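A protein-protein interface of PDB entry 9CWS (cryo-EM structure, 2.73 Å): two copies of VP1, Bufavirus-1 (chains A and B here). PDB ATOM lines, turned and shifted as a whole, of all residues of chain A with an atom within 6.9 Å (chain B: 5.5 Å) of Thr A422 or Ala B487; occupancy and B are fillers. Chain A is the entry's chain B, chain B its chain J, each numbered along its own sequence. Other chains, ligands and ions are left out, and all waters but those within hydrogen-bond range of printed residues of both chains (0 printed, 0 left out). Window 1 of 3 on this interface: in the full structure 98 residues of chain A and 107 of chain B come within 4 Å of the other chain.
Thr A422 touches just one residue of chain B: Ala B487. His A424 touches none of the printed residues of chain B. Of the printed residues of chain B, His A469 touches His B480, Ile B488 and Asn B489. Of the printed residues of chain A, Gly B485 touches Arg A423 (3.5 Å). Of the printed residues of chain A, Ala B487 touches Thr A422 and Ala A462. The nearest residue of chain B that does not touch Thr A422 is His B480 (5.4 Å). The nearest printed residue of chain B that does not touch Trp A452 is Asn B489 (5.9 Å).
NH1 of Arg A423 lies within hydrogen-bond range of O of Pro B486, 2.7 Å away. The side-chain amide nitrogen of Asn B489 lies within hydrogen-bond range of a ring nitrogen (ND1) of His A469 (3.4 Å).
The backbone NH of Trp A452 is in hydrogen-bond range of the backbone carbonyl oxygen of Thr A463 (3.0 Å). The indole nitrogen (NE1) of Trp A452 is in hydrogen-bond range of the backbone carbonyl oxygen (O) of Arg A464 (3.0 Å). The backbone NH (N) of Asn B489 sits at hydrogen-bond distance from the backbone carbonyl oxygen (O) of Arg B478 (3.0 Å). The backbone NH (N) of His B480 is in hydrogen-bond range of the backbone carbonyl oxygen (O) of Ala B487, at 2.7 Å.
No position is printed for both chains.
OG1 of Thr A422 touches CB of Ala B487, at 3.2 Å. Gly B485 touches Arg A423. Trp A452 touches Ile B488 (CD1 to CB, 3.7 Å). Pro B486 touches Ala A462 (O to CB, 3.2 Å). O of Ala A462 touches CA of Ala B487, at 3.5 Å. Ile B488 touches Ala A462 (N to O, 3.6 Å). Thr A463 touches Ile B488. His B480 touches His A469 (ND1 to CE1, 3.4 Å). CD2 of His A469 touches O of Ile B488 (3.4 Å).
Hydrophobic or aromatic side chains of chain A within 4 Å of the printed part of chain B: Trp A452, Ala A462 and His A469. Along chain B the printed residues that touch a printed residue of chain A span positions 480 to 489.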
ATOM      1  N   GLN A 420      20.992   1.156   5.494  1.00  0.00           N
ATOM      2  CA  GLN A 420      19.783   0.839   6.239  1.00  0.00           C
ATOM      3  C   GLN A 420      18.603   1.666   5.757  1.00  0.00           C
ATOM      4  O   GLN A 420      18.701   2.889   5.635  1.00  0.00           O
ATOM      5  CB  GLN A 420      19.978   1.084   7.731  1.00  0.00           C
ATOM      6  CG  GLN A 420      20.882   0.132   8.445  1.00  0.00           C
ATOM      7  CD  GLN A 420      21.005   0.457   9.905  1.00  0.00           C
ATOM      8  OE1 GLN A 420      20.871   1.599  10.304  1.00  0.00           O
ATOM      9  NE2 GLN A 420      21.223  -0.552  10.719  1.00  0.00           N
ATOM     10  N   SER A 421      17.492   0.993   5.488  1.00  0.00           N
ATOM     11  CA  SER A 421      16.180   1.596   5.368  1.00  0.00           C
ATOM     12  C   SER A 421      15.452   1.415   6.702  1.00  0.00           C
ATOM     13  O   SER A 421      16.052   0.988   7.689  1.00  0.00           O
ATOM     14  CB  SER A 421      15.442   0.981   4.179  1.00  0.00           C
ATOM     15  OG  SER A 421      15.217  -0.398   4.362  1.00  0.00           O
ATOM     16  N   THR A 422      14.167   1.751   6.756  1.00  0.00           N
ATOM     17  CA  THR A 422      13.443   1.567   8.007  1.00  0.00           C
ATOM     18  C   THR A 422      13.177   0.107   8.323  1.00  0.00           C
ATOM     19  O   THR A 422      12.824  -0.207   9.463  1.00  0.00           O
ATOM     20  CB  THR A 422      12.120   2.328   7.994  1.00  0.00           C
ATOM     21  OG1 THR A 422      11.294   1.843   6.938  1.00  0.00           O
ATOM     22  CG2 THR A 422      12.380   3.765   7.770  1.00  0.00           C
ATOM     23  N   ARG A 423      13.334  -0.782   7.353  1.00  0.00           N
ATOM     24  CA  ARG A 423      13.252  -2.213   7.579  1.00  0.00           C
ATOM     25  C   ARG A 423      14.556  -2.809   8.081  1.00  0.00           C
ATOM     26  O   ARG A 423      14.570  -3.971   8.485  1.00  0.00           O
ATOM     27  CB  ARG A 423      12.819  -2.912   6.291  1.00  0.00           C
ATOM     28  CG  ARG A 423      11.406  -2.598   5.854  1.00  0.00           C
ATOM     29  CD  ARG A 423      10.399  -3.196   6.805  1.00  0.00           C
ATOM     30  NE  ARG A 423      10.543  -4.642   6.878  1.00  0.00           N
ATOM     31  CZ  ARG A 423       9.946  -5.503   6.065  1.00  0.00           C
ATOM     32  NH1 ARG A 423       9.128  -5.076   5.125  1.00  0.00           N
ATOM     33  NH2 ARG A 423      10.156  -6.795   6.209  1.00  0.00           N
ATOM     34  N   HIS A 424      15.655  -2.055   8.023  1.00  0.00           N
ATOM     35  CA  HIS A 424      16.966  -2.473   8.506  1.00  0.00           C
ATOM     36  C   HIS A 424      17.312  -1.898   9.872  1.00  0.00           C
ATOM     37  O   HIS A 424      18.409  -2.148  10.373  1.00  0.00           O
ATOM     38  CB  HIS A 424      18.053  -2.061   7.520  1.00  0.00           C
ATOM     39  CG  HIS A 424      17.933  -2.697   6.178  1.00  0.00           C
ATOM     40  ND1 HIS A 424      18.313  -3.994   5.938  1.00  0.00           N
ATOM     41  CD2 HIS A 424      17.468  -2.216   5.004  1.00  0.00           C
ATOM     42  CE1 HIS A 424      18.097  -4.282   4.670  1.00  0.00           C
ATOM     43  NE2 HIS A 424      17.581  -3.223   4.083  1.00  0.00           N
ATOM     44  N   THR A 425      16.427  -1.121  10.482  1.00  0.00           N
ATOM     45  CA  THR A 425      16.908  -0.123  11.426  1.00  0.00           C
ATOM     46  C   THR A 425      16.768  -0.512  12.892  1.00  0.00           C
ATOM     47  O   THR A 425      17.769  -0.624  13.605  1.00  0.00           O
ATOM     48  CB  THR A 425      16.208   1.209  11.169  1.00  0.00           C
ATOM     49  OG1 THR A 425      16.439   1.603   9.815  1.00  0.00           O
ATOM     50  CG2 THR A 425      16.797   2.257  12.037  1.00  0.00           C
ATOM     51  N   GLY A 426      15.547  -0.702  13.365  1.00  0.00           N
ATOM     52  CA  GLY A 426      15.326  -0.816  14.792  1.00  0.00           C
ATOM     53  C   GLY A 426      15.360  -2.228  15.329  1.00  0.00           C
ATOM     54  O   GLY A 426      16.175  -3.045  14.899  1.00  0.00           O
ATOM     55  N   SER A 427      14.509  -2.506  16.309  1.00  0.00           N
ATOM     56  CA  SER A 427      14.361  -3.860  16.821  1.00  0.00           C
ATOM     57  C   SER A 427      13.941  -4.818  15.716  1.00  0.00           C
ATOM     58  O   SER A 427      13.268  -4.437  14.757  1.00  0.00           O
ATOM     59  CB  SER A 427      13.347  -3.883  17.960  1.00  0.00           C
ATOM     60  OG  SER A 427      12.080  -3.445  17.520  1.00  0.00           O
ATOM     61  N   TRP A 452       0.774  -0.172  13.254  1.00  0.00           N
ATOM     62  CA  TRP A 452       0.357   1.173  12.855  1.00  0.00           C
ATOM     63  C   TRP A 452      -1.144   1.376  12.984  1.00  0.00           C
ATOM     64  O   TRP A 452      -1.606   2.108  13.852  1.00  0.00           O
ATOM     65  CB  TRP A 452       0.817   1.533  11.440  1.00  0.00           C
ATOM     66  CG  TRP A 452       2.182   2.080  11.407  1.00  0.00           C
ATOM     67  CD1 TRP A 452       3.281   1.505  10.881  1.00  0.00           C
ATOM     68  CD2 TRP A 452       2.615   3.297  12.016  1.00  0.00           C
ATOM     69  NE1 TRP A 452       4.370   2.313  11.066  1.00  0.00           N
ATOM     70  CE2 TRP A 452       3.984   3.417  11.771  1.00  0.00           C
ATOM     71  CE3 TRP A 452       1.965   4.308  12.731  1.00  0.00           C
ATOM     72  CZ2 TRP A 452       4.724   4.500  12.216  1.00  0.00           C
ATOM     73  CZ3 TRP A 452       2.700   5.382  13.168  1.00  0.00           C
ATOM     74  CH2 TRP A 452       4.065   5.470  12.913  1.00  0.00           C
ATOM     75  N   ALA A 461       6.493  -7.222  10.288  1.00  0.00           N
ATOM     76  CA  ALA A 461       7.457  -6.142  10.463  1.00  0.00           C
ATOM     77  C   ALA A 461       7.216  -4.961   9.537  1.00  0.00           C
ATOM     78  O   ALA A 461       7.748  -3.878   9.791  1.00  0.00           O
ATOM     79  CB  ALA A 461       8.869  -6.667  10.240  1.00  0.00           C
ATOM     80  N   ALA A 462       6.452  -5.140   8.465  1.00  0.00           N
ATOM     81  CA  ALA A 462       6.179  -4.022   7.573  1.00  0.00           C
ATOM     82  C   ALA A 462       5.340  -2.945   8.247  1.00  0.00           C
ATOM     83  O   ALA A 462       5.555  -1.755   8.005  1.00  0.00           O
ATOM     84  CB  ALA A 462       5.482  -4.523   6.313  1.00  0.00           C
ATOM     85  N   THR A 463       4.383  -3.338   9.080  1.00  0.00           N
ATOM     86  CA  THR A 463       3.493  -2.407   9.754  1.00  0.00           C
ATOM     87  C   THR A 463       3.920  -2.068  11.178  1.00  0.00           C
ATOM     88  O   THR A 463       3.164  -1.404  11.887  1.00  0.00           O
ATOM     89  CB  THR A 463       2.071  -2.953   9.744  1.00  0.00           C
ATOM     90  OG1 THR A 463       2.055  -4.254  10.337  1.00  0.00           O
ATOM     91  CG2 THR A 463       1.567  -3.051   8.320  1.00  0.00           C
ATOM     92  N   ARG A 464       5.082  -2.533  11.625  1.00  0.00           N
ATOM     93  CA  ARG A 464       5.640  -2.076  12.889  1.00  0.00           C
ATOM     94  C   ARG A 464       5.767  -0.561  12.883  1.00  0.00           C
ATOM     95  O   ARG A 464       6.126   0.036  11.868  1.00  0.00           O
ATOM     96  CB  ARG A 464       7.018  -2.700  13.123  1.00  0.00           C
ATOM     97  CG  ARG A 464       7.660  -2.267  14.424  1.00  0.00           C
ATOM     98  CD  ARG A 464       9.011  -2.879  14.653  1.00  0.00           C
ATOM     99  NE  ARG A 464      10.054  -2.405  13.752  1.00  0.00           N
ATOM    100  CZ  ARG A 464      10.787  -1.320  13.961  1.00  0.00           C
ATOM    101  NH1 ARG A 464      11.726  -0.972  13.104  1.00  0.00           N
ATOM    102  NH2 ARG A 464      10.584  -0.579  15.026  1.00  0.00           N
ATOM    103  N   SER A 466       7.577   2.930  13.616  1.00  0.00           N
ATOM    104  CA  SER A 466       8.930   3.419  13.762  1.00  0.00           C
ATOM    105  C   SER A 466       8.850   4.870  14.193  1.00  0.00           C
ATOM    106  O   SER A 466       7.809   5.515  14.083  1.00  0.00           O
ATOM    107  CB  SER A 466       9.729   3.283  12.463  1.00  0.00           C
ATOM    108  OG  SER A 466       9.863   1.930  12.076  1.00  0.00           O
ATOM    109  N   PHE A 468      11.089   7.229  12.942  1.00  0.00           N
ATOM    110  CA  PHE A 468      11.477   8.052  11.816  1.00  0.00           C
ATOM    111  C   PHE A 468      11.254   7.251  10.546  1.00  0.00           C
ATOM    112  O   PHE A 468      10.807   6.105  10.586  1.00  0.00           O
ATOM    113  CB  PHE A 468      12.935   8.491  11.950  1.00  0.00           C
ATOM    114  CG  PHE A 468      13.283   9.002  13.318  1.00  0.00           C
ATOM    115  CD1 PHE A 468      12.798  10.203  13.774  1.00  0.00           C
ATOM    116  CD2 PHE A 468      14.128   8.291  14.133  1.00  0.00           C
ATOM    117  CE1 PHE A 468      13.127  10.668  15.025  1.00  0.00           C
ATOM    118  CE2 PHE A 468      14.459   8.761  15.379  1.00  0.00           C
ATOM    119  CZ  PHE A 468      13.956   9.948  15.818  1.00  0.00           C
ATOM    120  N   HIS A 469      11.557   7.851   9.403  1.00  0.00           N
ATOM    121  CA  HIS A 469      11.508   7.132   8.139  1.00  0.00           C
ATOM    122  C   HIS A 469      12.682   7.578   7.288  1.00  0.00           C
ATOM    123  O   HIS A 469      12.948   8.774   7.173  1.00  0.00           O
ATOM    124  CB  HIS A 469      10.185   7.355   7.407  1.00  0.00           C
ATOM    125  CG  HIS A 469       9.917   6.343   6.336  1.00  0.00           C
ATOM    126  ND1 HIS A 469      10.386   6.472   5.050  1.00  0.00           N
ATOM    127  CD2 HIS A 469       9.261   5.162   6.380  1.00  0.00           C
ATOM    128  CE1 HIS A 469      10.011   5.425   4.340  1.00  0.00           C
ATOM    129  NE2 HIS A 469       9.328   4.615   5.125  1.00  0.00           N
ATOM    130  N   ILE A 470      13.385   6.618   6.706  1.00  0.00           N
ATOM    131  CA  ILE A 470      14.603   6.891   5.958  1.00  0.00           C
ATOM    132  C   ILE A 470      14.250   6.994   4.482  1.00  0.00           C
ATOM    133  O   ILE A 470      13.770   6.033   3.878  1.00  0.00           O
ATOM    134  CB  ILE A 470      15.663   5.815   6.214  1.00  0.00           C
ATOM    135  CG1 ILE A 470      16.119   5.888   7.668  1.00  0.00           C
ATOM    136  CG2 ILE A 470      16.834   6.005   5.290  1.00  0.00           C
ATOM    137  CD1 ILE A 470      16.957   4.749   8.097  1.00  0.00           C
ATOM    138  N   GLY A 471      14.479   8.164   3.904  1.00  0.00           N
ATOM    139  CA  GLY A 471      14.193   8.419   2.513  1.00  0.00           C
ATOM    140  C   GLY A 471      12.824   9.042   2.311  1.00  0.00           C
ATOM    141  O   GLY A 471      11.965   9.039   3.192  1.00  0.00           O
ATOM    142  N   GLY A 541      19.087   1.949   0.657  1.00  0.00           N
ATOM    143  CA  GLY A 541      18.619   2.248   1.993  1.00  0.00           C
ATOM    144  C   GLY A 541      17.884   3.561   2.095  1.00  0.00           C
ATOM    145  O   GLY A 541      17.097   3.762   3.021  1.00  0.00           O
ATOM    146  N   ARG B 478       0.879   5.438   3.691  1.00  0.00           N
ATOM    147  CA  ARG B 478       1.870   5.304   2.636  1.00  0.00           C
ATOM    148  C   ARG B 478       2.659   4.024   2.863  1.00  0.00           C
ATOM    149  O   ARG B 478       3.199   3.819   3.949  1.00  0.00           O
ATOM    150  CB  ARG B 478       2.794   6.520   2.676  1.00  0.00           C
ATOM    151  CG  ARG B 478       3.902   6.560   1.669  1.00  0.00           C
ATOM    152  CD  ARG B 478       3.340   6.699   0.299  1.00  0.00           C
ATOM    153  NE  ARG B 478       4.364   6.999  -0.681  1.00  0.00           N
ATOM    154  CZ  ARG B 478       4.122   7.081  -1.976  1.00  0.00           C
ATOM    155  NH1 ARG B 478       5.087   7.384  -2.826  1.00  0.00           N
ATOM    156  NH2 ARG B 478       2.898   6.879  -2.418  1.00  0.00           N
ATOM    157  N   ILE B 479       2.727   3.165   1.852  1.00  0.00           N
ATOM    158  CA  ILE B 479       3.600   2.001   1.913  1.00  0.00           C
ATOM    159  C   ILE B 479       4.836   2.322   1.086  1.00  0.00           C
ATOM    160  O   ILE B 479       4.735   2.666  -0.090  1.00  0.00           O
ATOM    161  CB  ILE B 479       2.915   0.723   1.417  1.00  0.00           C
ATOM    162  CG1 ILE B 479       1.656   0.423   2.219  1.00  0.00           C
ATOM    163  CG2 ILE B 479       3.842  -0.439   1.604  1.00  0.00           C
ATOM    164  CD1 ILE B 479       0.391   0.712   1.488  1.00  0.00           C
ATOM    165  N   HIS B 480       6.010   2.199   1.706  1.00  0.00           N
ATOM    166  CA  HIS B 480       7.236   2.695   1.093  1.00  0.00           C
ATOM    167  C   HIS B 480       7.737   1.782  -0.018  1.00  0.00           C
ATOM    168  O   HIS B 480       8.047   2.257  -1.113  1.00  0.00           O
ATOM    169  CB  HIS B 480       8.302   2.866   2.166  1.00  0.00           C
ATOM    170  CG  HIS B 480       9.628   3.311   1.642  1.00  0.00           C
ATOM    171  ND1 HIS B 480       9.820   4.529   1.039  1.00  0.00           N
ATOM    172  CD2 HIS B 480      10.834   2.700   1.644  1.00  0.00           C
ATOM    173  CE1 HIS B 480      11.086   4.650   0.692  1.00  0.00           C
ATOM    174  NE2 HIS B 480      11.721   3.551   1.038  1.00  0.00           N
ATOM    175  N   TYR B 481       7.836   0.478   0.236  1.00  0.00           N
ATOM    176  CA  TYR B 481       8.474  -0.469  -0.687  1.00  0.00           C
ATOM    177  C   TYR B 481       9.880  -0.007  -1.076  1.00  0.00           C
ATOM    178  O   TYR B 481      10.145   0.397  -2.202  1.00  0.00           O
ATOM    179  CB  TYR B 481       7.638  -0.715  -1.950  1.00  0.00           C
ATOM    180  CG  TYR B 481       6.405  -1.555  -1.745  1.00  0.00           C
ATOM    181  CD1 TYR B 481       6.490  -2.935  -1.685  1.00  0.00           C
ATOM    182  CD2 TYR B 481       5.156  -0.974  -1.657  1.00  0.00           C
ATOM    183  CE1 TYR B 481       5.371  -3.708  -1.504  1.00  0.00           C
ATOM    184  CE2 TYR B 481       4.033  -1.740  -1.484  1.00  0.00           C
ATOM    185  CZ  TYR B 481       4.144  -3.104  -1.403  1.00  0.00           C
ATOM    186  OH  TYR B 481       3.020  -3.866  -1.227  1.00  0.00           O
ATOM    187  N   GLY B 482      10.778  -0.084  -0.103  1.00  0.00           N
ATOM    188  CA  GLY B 482      12.165   0.244  -0.350  1.00  0.00           C
ATOM    189  C   GLY B 482      13.036  -0.987  -0.397  1.00  0.00           C
ATOM    190  O   GLY B 482      12.533  -2.091  -0.614  1.00  0.00           O
ATOM    191  N   GLY B 485      12.185  -4.122   1.957  1.00  0.00           N
ATOM    192  CA  GLY B 485      10.784  -4.436   1.869  1.00  0.00           C
ATOM    193  C   GLY B 485       9.888  -3.269   2.196  1.00  0.00           C
ATOM    194  O   GLY B 485      10.345  -2.173   2.516  1.00  0.00           O
ATOM    195  N   PRO B 486       8.579  -3.489   2.117  1.00  0.00           N
ATOM    196  CA  PRO B 486       7.631  -2.406   2.380  1.00  0.00           C
ATOM    197  C   PRO B 486       7.608  -2.010   3.848  1.00  0.00           C
ATOM    198  O   PRO B 486       7.673  -2.851   4.742  1.00  0.00           O
ATOM    199  CB  PRO B 486       6.292  -3.003   1.937  1.00  0.00           C
ATOM    200  CG  PRO B 486       6.474  -4.455   2.072  1.00  0.00           C
ATOM    201  CD  PRO B 486       7.895  -4.727   1.711  1.00  0.00           C
ATOM    202  N   ALA B 487       7.527  -0.708   4.086  1.00  0.00           N
ATOM    203  CA  ALA B 487       7.278  -0.175   5.413  1.00  0.00           C
ATOM    204  C   ALA B 487       6.240   0.925   5.291  1.00  0.00           C
ATOM    205  O   ALA B 487       5.818   1.254   4.184  1.00  0.00           O
ATOM    206  CB  ALA B 487       8.562   0.353   6.045  1.00  0.00           C
ATOM    207  N   ILE B 488       5.827   1.510   6.404  1.00  0.00           N
ATOM    208  CA  ILE B 488       4.840   2.577   6.361  1.00  0.00           C
ATOM    209  C   ILE B 488       5.502   3.903   6.683  1.00  0.00           C
ATOM    210  O   ILE B 488       6.284   4.007   7.632  1.00  0.00           O
ATOM    211  CB  ILE B 488       3.663   2.286   7.308  1.00  0.00           C
ATOM    212  CG1 ILE B 488       2.790   1.192   6.705  1.00  0.00           C
ATOM    213  CG2 ILE B 488       2.867   3.540   7.603  1.00  0.00           C
ATOM    214  CD1 ILE B 488       1.759   0.698   7.611  1.00  0.00           C
ATOM    215  N   ASN B 489       5.211   4.910   5.879  1.00  0.00           N
ATOM    216  CA  ASN B 489       5.676   6.261   6.113  1.00  0.00           C
ATOM    217  C   ASN B 489       4.553   7.005   6.826  1.00  0.00           C
ATOM    218  O   ASN B 489       3.511   7.262   6.213  1.00  0.00           O
ATOM    219  CB  ASN B 489       6.050   6.899   4.784  1.00  0.00           C
ATOM    220  CG  ASN B 489       6.934   8.098   4.943  1.00  0.00           C
ATOM    221  OD1 ASN B 489       6.906   8.781   5.957  1.00  0.00           O
ATOM    222  ND2 ASN B 489       7.783   8.318   3.967  1.00  0.00           N
